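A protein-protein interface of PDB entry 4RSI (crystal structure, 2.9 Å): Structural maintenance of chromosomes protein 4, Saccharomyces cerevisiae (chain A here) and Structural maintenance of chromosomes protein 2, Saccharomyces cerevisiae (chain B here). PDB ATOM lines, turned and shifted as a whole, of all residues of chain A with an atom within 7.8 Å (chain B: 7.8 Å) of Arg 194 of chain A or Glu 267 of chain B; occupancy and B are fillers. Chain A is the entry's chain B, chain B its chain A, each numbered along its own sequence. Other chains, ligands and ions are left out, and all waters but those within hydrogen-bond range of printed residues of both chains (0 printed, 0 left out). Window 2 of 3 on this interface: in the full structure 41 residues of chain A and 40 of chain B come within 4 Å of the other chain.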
ATOM      1  N   ARG A 158       9.053  15.358  23.343  1.00  0.00           N
ATOM      2  CA  ARG A 158       9.851  15.291  22.123  1.00  0.00           C
ATOM      3  C   ARG A 158       9.101  14.554  21.022  1.00  0.00           C
ATOM      4  O   ARG A 158       9.479  14.594  19.866  1.00  0.00           O
ATOM      5  CB  ARG A 158      11.195  14.607  22.373  1.00  0.00           C
ATOM      6  CG  ARG A 158      12.192  15.383  23.253  1.00  0.00           C
ATOM      7  CD  ARG A 158      13.207  16.177  22.433  1.00  0.00           C
ATOM      8  NE  ARG A 158      13.987  15.377  21.482  1.00  0.00           N
ATOM      9  CZ  ARG A 158      14.861  14.417  21.806  1.00  0.00           C
ATOM     10  NH1 ARG A 158      15.068  14.064  23.084  1.00  0.00           N
ATOM     11  NH2 ARG A 158      15.523  13.791  20.836  1.00  0.00           N
ATOM     12  N   ASP A 161       8.876  16.352  17.880  1.00  0.00           N
ATOM     13  CA  ASP A 161       9.984  16.501  16.925  1.00  0.00           C
ATOM     14  C   ASP A 161       9.586  16.052  15.537  1.00  0.00           C
ATOM     15  O   ASP A 161       8.587  15.379  15.365  1.00  0.00           O
ATOM     16  CB  ASP A 161      11.213  15.697  17.358  1.00  0.00           C
ATOM     17  CG  ASP A 161      11.799  16.195  18.669  1.00  0.00           C
ATOM     18  OD1 ASP A 161      11.363  17.284  19.122  1.00  0.00           O
ATOM     19  OD2 ASP A 161      12.687  15.503  19.242  1.00  0.00           O
ATOM     20  N   PHE A 187      14.141  18.810  14.772  1.00  0.00           N
ATOM     21  CA  PHE A 187      14.320  17.674  13.869  1.00  0.00           C
ATOM     22  C   PHE A 187      15.162  16.552  14.450  1.00  0.00           C
ATOM     23  O   PHE A 187      16.276  16.770  14.927  1.00  0.00           O
ATOM     24  CB  PHE A 187      14.879  18.128  12.532  1.00  0.00           C
ATOM     25  CG  PHE A 187      13.978  19.089  11.803  1.00  0.00           C
ATOM     26  CD1 PHE A 187      13.013  18.620  10.925  1.00  0.00           C
ATOM     27  CD2 PHE A 187      14.068  20.459  12.006  1.00  0.00           C
ATOM     28  CE1 PHE A 187      12.146  19.509  10.232  1.00  0.00           C
ATOM     29  CE2 PHE A 187      13.205  21.347  11.319  1.00  0.00           C
ATOM     30  CZ  PHE A 187      12.245  20.860  10.429  1.00  0.00           C
ATOM     31  N   ILE A 188      14.576  15.355  14.443  1.00  0.00           N
ATOM     32  CA  ILE A 188      15.267  14.138  14.809  1.00  0.00           C
ATOM     33  C   ILE A 188      15.957  13.699  13.537  1.00  0.00           C
ATOM     34  O   ILE A 188      15.284  13.374  12.549  1.00  0.00           O
ATOM     35  CB  ILE A 188      14.281  13.037  15.234  1.00  0.00           C
ATOM     36  CG1 ILE A 188      13.778  13.268  16.657  1.00  0.00           C
ATOM     37  CG2 ILE A 188      14.934  11.667  15.148  1.00  0.00           C
ATOM     38  CD1 ILE A 188      14.605  12.549  17.737  1.00  0.00           C
ATOM     39  N   LEU A 189      17.289  13.722  13.539  1.00  0.00           N
ATOM     40  CA  LEU A 189      18.070  13.345  12.358  1.00  0.00           C
ATOM     41  C   LEU A 189      18.430  11.861  12.431  1.00  0.00           C
ATOM     42  O   LEU A 189      19.108  11.420  13.375  1.00  0.00           O
ATOM     43  CB  LEU A 189      19.334  14.190  12.279  1.00  0.00           C
ATOM     44  CG  LEU A 189      19.064  15.690  12.311  1.00  0.00           C
ATOM     45  CD1 LEU A 189      20.366  16.467  12.447  1.00  0.00           C
ATOM     46  CD2 LEU A 189      18.305  16.104  11.062  1.00  0.00           C
ATOM     47  N   LEU A 190      17.975  11.088  11.447  1.00  0.00           N
ATOM     48  CA  LEU A 190      18.159   9.642  11.504  1.00  0.00           C
ATOM     49  C   LEU A 190      19.629   9.204  11.291  1.00  0.00           C
ATOM     50  O   LEU A 190      20.139   8.372  12.061  1.00  0.00           O
ATOM     51  CB  LEU A 190      17.178   8.943  10.555  1.00  0.00           C
ATOM     52  CG  LEU A 190      15.708   9.026  10.999  1.00  0.00           C
ATOM     53  CD1 LEU A 190      14.732   8.638   9.884  1.00  0.00           C
ATOM     54  CD2 LEU A 190      15.465   8.168  12.244  1.00  0.00           C
ATOM     55  N   ASP A 191      20.299   9.788  10.283  1.00  0.00           N
ATOM     56  CA  ASP A 191      21.726   9.520   9.976  1.00  0.00           C
ATOM     57  C   ASP A 191      22.649   9.612  11.184  1.00  0.00           C
ATOM     58  O   ASP A 191      23.191   8.612  11.661  1.00  0.00           O
ATOM     59  CB  ASP A 191      22.268  10.510   8.928  1.00  0.00           C
ATOM     60  CG  ASP A 191      21.178  11.104   8.050  1.00  0.00           C
ATOM     61  OD1 ASP A 191      20.082  10.497   7.999  1.00  0.00           O
ATOM     62  OD2 ASP A 191      21.415  12.173   7.418  1.00  0.00           O
ATOM     63  N   ARG A 192      22.820  10.842  11.661  1.00  0.00           N
ATOM     64  CA  ARG A 192      23.668  11.149  12.809  1.00  0.00           C
ATOM     65  C   ARG A 192      23.169  10.526  14.119  1.00  0.00           C
ATOM     66  O   ARG A 192      23.811  10.640  15.161  1.00  0.00           O
ATOM     67  CB  ARG A 192      23.786  12.665  12.977  1.00  0.00           C
ATOM     68  CG  ARG A 192      25.173  13.137  13.385  1.00  0.00           C
ATOM     69  CD  ARG A 192      26.163  13.227  12.234  1.00  0.00           C
ATOM     70  NE  ARG A 192      27.495  13.617  12.686  1.00  0.00           N
ATOM     71  CZ  ARG A 192      28.564  13.657  11.905  1.00  0.00           C
ATOM     72  NH1 ARG A 192      28.463  13.333  10.622  1.00  0.00           N
ATOM     73  NH2 ARG A 192      29.739  14.024  12.401  1.00  0.00           N
ATOM     74  N   LEU A 193      22.028   9.857  14.073  1.00  0.00           N
ATOM     75  CA  LEU A 193      21.434   9.338  15.289  1.00  0.00           C
ATOM     76  C   LEU A 193      22.211   8.143  15.805  1.00  0.00           C
ATOM     77  O   LEU A 193      22.477   7.229  15.037  1.00  0.00           O
ATOM     78  CB  LEU A 193      20.002   8.924  15.007  1.00  0.00           C
ATOM     79  CG  LEU A 193      19.049   9.311  16.117  1.00  0.00           C
ATOM     80  CD1 LEU A 193      17.650   9.454  15.525  1.00  0.00           C
ATOM     81  CD2 LEU A 193      19.121   8.252  17.224  1.00  0.00           C
ATOM     82  N   ARG A 194      22.568   8.143  17.092  1.00  0.00           N
ATOM     83  CA  ARG A 194      23.284   7.007  17.699  1.00  0.00           C
ATOM     84  C   ARG A 194      22.541   5.694  17.464  1.00  0.00           C
ATOM     85  O   ARG A 194      21.309   5.680  17.371  1.00  0.00           O
ATOM     86  CB  ARG A 194      23.489   7.224  19.209  1.00  0.00           C
ATOM     87  CG  ARG A 194      23.707   5.945  20.057  1.00  0.00           C
ATOM     88  CD  ARG A 194      25.171   5.737  20.371  1.00  0.00           C
ATOM     89  NE  ARG A 194      25.477   5.680  21.807  1.00  0.00           N
ATOM     90  CZ  ARG A 194      25.680   6.740  22.599  1.00  0.00           C
ATOM     91  NH1 ARG A 194      25.575   7.980  22.122  1.00  0.00           N
ATOM     92  NH2 ARG A 194      25.969   6.555  23.887  1.00  0.00           N
ATOM     93  N   GLN A 195      23.290   4.598  17.338  1.00  0.00           N
ATOM     94  CA  GLN A 195      22.697   3.261  17.193  1.00  0.00           C
ATOM     95  C   GLN A 195      22.560   2.524  18.546  1.00  0.00           C
ATOM     96  O   GLN A 195      23.562   2.065  19.144  1.00  0.00           O
ATOM     97  CB  GLN A 195      23.495   2.419  16.201  1.00  0.00           C
ATOM     98  CG  GLN A 195      22.647   1.420  15.462  1.00  0.00           C
ATOM     99  CD  GLN A 195      21.609   2.079  14.588  1.00  0.00           C
ATOM    100  OE1 GLN A 195      21.784   3.212  14.137  1.00  0.00           O
ATOM    101  NE2 GLN A 195      20.513   1.369  14.339  1.00  0.00           N
ATOM    102  N   PHE A 196      21.309   2.408  19.000  1.00  0.00           N
ATOM    103  CA  PHE A 196      20.987   1.994  20.364  1.00  0.00           C
ATOM    104  C   PHE A 196      20.646   0.502  20.524  1.00  0.00           C
ATOM    105  O   PHE A 196      20.200  -0.151  19.575  1.00  0.00           O
ATOM    106  CB  PHE A 196      19.804   2.827  20.871  1.00  0.00           C
ATOM    107  CG  PHE A 196      20.169   4.209  21.358  1.00  0.00           C
ATOM    108  CD1 PHE A 196      21.012   4.387  22.457  1.00  0.00           C
ATOM    109  CD2 PHE A 196      19.617   5.328  20.764  1.00  0.00           C
ATOM    110  CE1 PHE A 196      21.334   5.643  22.924  1.00  0.00           C
ATOM    111  CE2 PHE A 196      19.925   6.598  21.231  1.00  0.00           C
ATOM    112  CZ  PHE A 196      20.789   6.752  22.311  1.00  0.00           C
ATOM    113  N   ASN A 197      20.820  -0.010  21.744  1.00  0.00           N
ATOM    114  CA  ASN A 197      20.410  -1.363  22.100  1.00  0.00           C
ATOM    115  C   ASN A 197      18.947  -1.465  22.506  1.00  0.00           C
ATOM    116  O   ASN A 197      18.623  -1.407  23.693  1.00  0.00           O
ATOM    117  CB  ASN A 197      21.268  -1.864  23.252  1.00  0.00           C
ATOM    118  CG  ASN A 197      22.723  -1.710  22.967  1.00  0.00           C
ATOM    119  OD1 ASN A 197      23.096  -0.966  22.064  1.00  0.00           O
ATOM    120  ND2 ASN A 197      23.565  -2.415  23.714  1.00  0.00           N
ATOM    121  N   LEU A 198      18.069  -1.665  21.529  1.00  0.00           N
ATOM    122  CA  LEU A 198      16.633  -1.719  21.790  1.00  0.00           C
ATOM    123  C   LEU A 198      16.162  -2.994  22.509  1.00  0.00           C
ATOM    124  O   LEU A 198      14.987  -3.348  22.441  1.00  0.00           O
ATOM    125  CB  LEU A 198      15.854  -1.581  20.485  1.00  0.00           C
ATOM    126  CG  LEU A 198      16.253  -0.545  19.435  1.00  0.00           C
ATOM    127  CD1 LEU A 198      15.123  -0.433  18.432  1.00  0.00           C
ATOM    128  CD2 LEU A 198      16.567   0.816  20.030  1.00  0.00           C
ATOM    129  N   ASN A 223      14.673   3.140  16.518  1.00  0.00           N
ATOM    130  CA  ASN A 223      15.814   3.682  17.234  1.00  0.00           C
ATOM    131  C   ASN A 223      15.456   5.058  17.762  1.00  0.00           C
ATOM    132  O   ASN A 223      15.743   5.388  18.915  1.00  0.00           O
ATOM    133  CB  ASN A 223      17.077   3.722  16.368  1.00  0.00           C
ATOM    134  CG  ASN A 223      18.336   3.412  17.169  1.00  0.00           C
ATOM    135  OD1 ASN A 223      18.261   2.859  18.275  1.00  0.00           O
ATOM    136  ND2 ASN A 223      19.497   3.767  16.616  1.00  0.00           N
ATOM    137  N   ALA A 224      14.805   5.842  16.908  1.00  0.00           N
ATOM    138  CA  ALA A 224      14.309   7.170  17.267  1.00  0.00           C
ATOM    139  C   ALA A 224      13.534   7.122  18.576  1.00  0.00           C
ATOM    140  O   ALA A 224      13.911   7.771  19.548  1.00  0.00           O
ATOM    141  CB  ALA A 224      13.437   7.718  16.159  1.00  0.00           C
ATOM    142  N   TYR A 226      13.782   5.126  20.769  1.00  0.00           N
ATOM    143  CA  TYR A 226      14.633   4.931  21.922  1.00  0.00           C
ATOM    144  C   TYR A 226      15.523   6.150  22.176  1.00  0.00           C
ATOM    145  O   TYR A 226      16.156   6.251  23.228  1.00  0.00           O
ATOM    146  CB  TYR A 226      15.437   3.639  21.850  1.00  0.00           C
ATOM    147  CG  TYR A 226      16.081   3.280  23.169  1.00  0.00           C
ATOM    148  CD1 TYR A 226      15.378   2.612  24.154  1.00  0.00           C
ATOM    149  CD2 TYR A 226      17.386   3.627  23.434  1.00  0.00           C
ATOM    150  CE1 TYR A 226      15.975   2.294  25.374  1.00  0.00           C
ATOM    151  CE2 TYR A 226      17.984   3.319  24.640  1.00  0.00           C
ATOM    152  CZ  TYR A 226      17.288   2.647  25.606  1.00  0.00           C
ATOM    153  OH  TYR A 226      17.918   2.346  26.804  1.00  0.00           O
ATOM    154  N   SER A 227      15.563   7.086  21.228  1.00  0.00           N
ATOM    155  CA  SER A 227      16.342   8.314  21.419  1.00  0.00           C
ATOM    156  C   SER A 227      15.611   9.283  22.363  1.00  0.00           C
ATOM    157  O   SER A 227      16.243  10.024  23.125  1.00  0.00           O
ATOM    158  CB  SER A 227      16.645   8.981  20.077  1.00  0.00           C
ATOM    159  OG  SER A 227      17.281  10.235  20.256  1.00  0.00           O
ATOM    160  N   ARG A 230      13.991   6.340  27.133  1.00  0.00           N
ATOM    161  CA  ARG A 230      15.077   5.396  27.343  1.00  0.00           C
ATOM    162  C   ARG A 230      15.164   5.052  28.800  1.00  0.00           C
ATOM    163  O   ARG A 230      15.507   5.911  29.609  1.00  0.00           O
ATOM    164  CB  ARG A 230      16.437   5.937  26.847  1.00  0.00           C
ATOM    165  CG  ARG A 230      16.606   7.445  26.707  1.00  0.00           C
ATOM    166  CD  ARG A 230      17.441   7.759  25.445  1.00  0.00           C
ATOM    167  NE  ARG A 230      18.740   8.419  25.648  1.00  0.00           N
ATOM    168  CZ  ARG A 230      19.729   7.978  26.434  1.00  0.00           C
ATOM    169  NH1 ARG A 230      19.595   6.866  27.161  1.00  0.00           N
ATOM    170  NH2 ARG A 230      20.862   8.672  26.502  1.00  0.00           N
ATOM    171  N   THR B 247      30.106  21.023  17.240  1.00  0.00           N
ATOM    172  CA  THR B 247      29.290  19.963  17.835  1.00  0.00           C
ATOM    173  C   THR B 247      29.669  18.610  17.259  1.00  0.00           C
ATOM    174  O   THR B 247      30.012  17.661  17.988  1.00  0.00           O
ATOM    175  CB  THR B 247      27.775  20.193  17.580  1.00  0.00           C
ATOM    176  OG1 THR B 247      27.257  21.135  18.529  1.00  0.00           O
ATOM    177  CG2 THR B 247      26.983  18.895  17.721  1.00  0.00           C
ATOM    178  N   PHE B 248      29.588  18.531  15.937  1.00  0.00           N
ATOM    179  CA  PHE B 248      29.937  17.317  15.248  1.00  0.00           C
ATOM    180  C   PHE B 248      31.422  17.423  14.933  1.00  0.00           C
ATOM    181  O   PHE B 248      31.805  17.907  13.864  1.00  0.00           O
ATOM    182  CB  PHE B 248      29.065  17.151  13.998  1.00  0.00           C
ATOM    183  CG  PHE B 248      27.584  16.975  14.304  1.00  0.00           C
ATOM    184  CD1 PHE B 248      27.167  16.297  15.454  1.00  0.00           C
ATOM    185  CD2 PHE B 248      26.608  17.483  13.445  1.00  0.00           C
ATOM    186  CE1 PHE B 248      25.787  16.129  15.746  1.00  0.00           C
ATOM    187  CE2 PHE B 248      25.229  17.321  13.723  1.00  0.00           C
ATOM    188  CZ  PHE B 248      24.821  16.641  14.874  1.00  0.00           C
ATOM    189  N   ARG B 253      32.204  16.832  21.605  1.00  0.00           N
ATOM    190  CA  ARG B 253      30.814  16.579  21.280  1.00  0.00           C
ATOM    191  C   ARG B 253      29.918  17.300  22.265  1.00  0.00           C
ATOM    192  O   ARG B 253      29.497  16.746  23.281  1.00  0.00           O
ATOM    193  CB  ARG B 253      30.523  15.089  21.129  1.00  0.00           C
ATOM    194  CG  ARG B 253      30.911  14.583  19.740  1.00  0.00           C
ATOM    195  CD  ARG B 253      30.704  13.104  19.570  1.00  0.00           C
ATOM    196  NE  ARG B 253      29.330  12.688  19.833  1.00  0.00           N
ATOM    197  CZ  ARG B 253      28.387  12.584  18.902  1.00  0.00           C
ATOM    198  NH1 ARG B 253      27.167  12.189  19.251  1.00  0.00           N
ATOM    199  NH2 ARG B 253      28.663  12.870  17.632  1.00  0.00           N
ATOM    200  N   ALA B 254      29.663  18.563  21.941  1.00  0.00           N
ATOM    201  CA  ALA B 254      28.965  19.474  22.825  1.00  0.00           C
ATOM    202  C   ALA B 254      27.736  20.065  22.134  1.00  0.00           C
ATOM    203  O   ALA B 254      27.661  20.109  20.913  1.00  0.00           O
ATOM    204  CB  ALA B 254      29.914  20.572  23.269  1.00  0.00           C
ATOM    205  N   TYR B 264      22.332  22.743  17.604  1.00  0.00           N
ATOM    206  CA  TYR B 264      22.902  21.537  17.038  1.00  0.00           C
ATOM    207  C   TYR B 264      23.292  20.694  18.244  1.00  0.00           C
ATOM    208  O   TYR B 264      24.187  21.068  19.018  1.00  0.00           O
ATOM    209  CB  TYR B 264      24.111  21.850  16.121  1.00  0.00           C
ATOM    210  CG  TYR B 264      23.779  22.707  14.899  1.00  0.00           C
ATOM    211  CD1 TYR B 264      23.278  23.983  15.053  1.00  0.00           C
ATOM    212  CD2 TYR B 264      23.970  22.249  13.610  1.00  0.00           C
ATOM    213  CE1 TYR B 264      22.956  24.786  13.972  1.00  0.00           C
ATOM    214  CE2 TYR B 264      23.651  23.054  12.495  1.00  0.00           C
ATOM    215  CZ  TYR B 264      23.139  24.334  12.691  1.00  0.00           C
ATOM    216  OH  TYR B 264      22.801  25.192  11.638  1.00  0.00           O
ATOM    217  N   ASP B 265      22.572  19.585  18.424  1.00  0.00           N
ATOM    218  CA  ASP B 265      22.758  18.668  19.555  1.00  0.00           C
ATOM    219  C   ASP B 265      23.370  17.413  19.003  1.00  0.00           C
ATOM    220  O   ASP B 265      22.876  16.885  18.012  1.00  0.00           O
ATOM    221  CB  ASP B 265      21.401  18.323  20.193  1.00  0.00           C
ATOM    222  CG  ASP B 265      21.528  17.805  21.632  1.00  0.00           C
ATOM    223  OD1 ASP B 265      22.405  16.947  21.904  1.00  0.00           O
ATOM    224  OD2 ASP B 265      20.746  18.268  22.500  1.00  0.00           O
ATOM    225  N   PRO B 266      24.450  16.923  19.631  1.00  0.00           N
ATOM    226  CA  PRO B 266      25.128  15.719  19.128  1.00  0.00           C
ATOM    227  C   PRO B 266      24.322  14.432  19.364  1.00  0.00           C
ATOM    228  O   PRO B 266      24.880  13.421  19.796  1.00  0.00           O
ATOM    229  CB  PRO B 266      26.460  15.705  19.905  1.00  0.00           C
ATOM    230  CG  PRO B 266      26.189  16.473  21.151  1.00  0.00           C
ATOM    231  CD  PRO B 266      25.157  17.523  20.776  1.00  0.00           C
ATOM    232  N   GLU B 267      23.026  14.483  19.082  1.00  0.00           N
ATOM    233  CA  GLU B 267      22.167  13.336  19.256  1.00  0.00           C
ATOM    234  C   GLU B 267      21.107  13.331  18.170  1.00  0.00           C
ATOM    235  O   GLU B 267      19.948  13.008  18.415  1.00  0.00           O
ATOM    236  CB  GLU B 267      21.526  13.340  20.652  1.00  0.00           C
ATOM    237  CG  GLU B 267      22.476  13.022  21.809  1.00  0.00           C
ATOM    238  CD  GLU B 267      23.006  11.575  21.786  1.00  0.00           C
ATOM    239  OE1 GLU B 267      23.587  11.144  20.762  1.00  0.00           O
ATOM    240  OE2 GLU B 267      22.850  10.858  22.805  1.00  0.00           O
ATOM    241  N   GLY B 268      21.514  13.692  16.964  1.00  0.00           N
ATOM    242  CA  GLY B 268      20.611  13.688  15.831  1.00  0.00           C
ATOM    243  C   GLY B 268      19.536  14.745  15.956  1.00  0.00           C
ATOM    244  O   GLY B 268      18.422  14.562  15.464  1.00  0.00           O
ATOM    245  N   THR B 269      19.865  15.850  16.619  1.00  0.00           N
ATOM    246  CA  THR B 269      18.899  16.921  16.836  1.00  0.00           C
ATOM    247  C   THR B 269      19.369  18.232  16.219  1.00  0.00           C
ATOM    248  O   THR B 269      20.464  18.698  16.515  1.00  0.00           O
ATOM    249  CB  THR B 269      18.661  17.180  18.342  1.00  0.00           C
ATOM    250  OG1 THR B 269      18.581  15.946  19.056  1.00  0.00           O
ATOM    251  CG2 THR B 269      17.386  17.927  18.545  1.00  0.00           C
ATOM    252  N   LEU B 270      18.535  18.831  15.376  1.00  0.00           N
ATOM    253  CA  LEU B 270      18.791  20.173  14.878  1.00  0.00           C
ATOM    254  C   LEU B 270      17.515  20.999  14.922  1.00  0.00           C
ATOM    255  O   LEU B 270      16.550  20.683  14.227  1.00  0.00           O
ATOM    256  CB  LEU B 270      19.308  20.132  13.439  1.00  0.00           C
ATOM    257  CG  LEU B 270      19.108  21.429  12.622  1.00  0.00           C
ATOM    258  CD1 LEU B 270      20.168  22.494  12.903  1.00  0.00           C
ATOM    259  CD2 LEU B 270      19.006  21.164  11.129  1.00  0.00           C
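The guanidinium group (NH1) of Arg 194 of chain A lies within salt-bridge range of the side-chain carboxylate (OE1) of Glu 267 of chain B (3.98 Å).
N of Leu 270 of chain B is in hydrogen-bond range of O of Phe 187 of chain A, 3.1 Å away.
O of Phe 187 of chain A lies close to O of Gly 268 of chain B (3.1 Å).
The backbone NH of Leu 189 of chain A sits close to the backbone carbonyl oxygen of Gly 268 of chain B.
Of the 11 printed residues of chain B, 5 touch a printed residue of chain A.
Hydrophobic or aromatic side chains of chain B that line the printed part of chain A: Phe 248 and Leu 270.
Of the 19 printed residues of chain A, 5 touch a printed residue of chain B.
Hydrophobic or aromatic side chains of chain A that line the printed part of chain B: Phe 187 and Leu 189.
Along chain A the printed residues that touch a printed residue of chain B span positions 187 to 194.
Phe 187 of chain A touches Thr 269 of chain B.
C of Ile 188 of chain A touches O of Gly 268 of chain B (3.2 Å).
CB of Leu 270 of chain B touches CD1 of Leu 189 of chain A, 3.9 Å away.
NH2 of Arg 192 of chain A touches CB of Phe 248 of chain B, at 3.6 Å.
Of chain B, only Glu 267 (3.98 Å) comes within 4 Å of Arg 194 of chain A.
Of chain A, only Phe 187, Ile 188 and Leu 189 come within 4 Å of Gly 268 of chain B.
Of the printed residues of chain B, Ile 188 of chain A touches Gly 268 (3.2 Å).
Of the printed residues of chain B, Phe 187 of chain A touches Gly 268, Thr 269 and Leu 270.
The nearest residue of chain B that does not touch Arg 194 of chain A is Arg 253 of chain B (5.3 Å).
The backbone carbonyl oxygen of Glu 267 of chain B is in hydrogen-bond range of the side-chain hydroxyl of Thr 269 of chain B, 3.3 Å away.
O of Arg 194 of chain A lies within hydrogen-bond range of ND2 of Asn 223 of chain A (2.7 Å).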
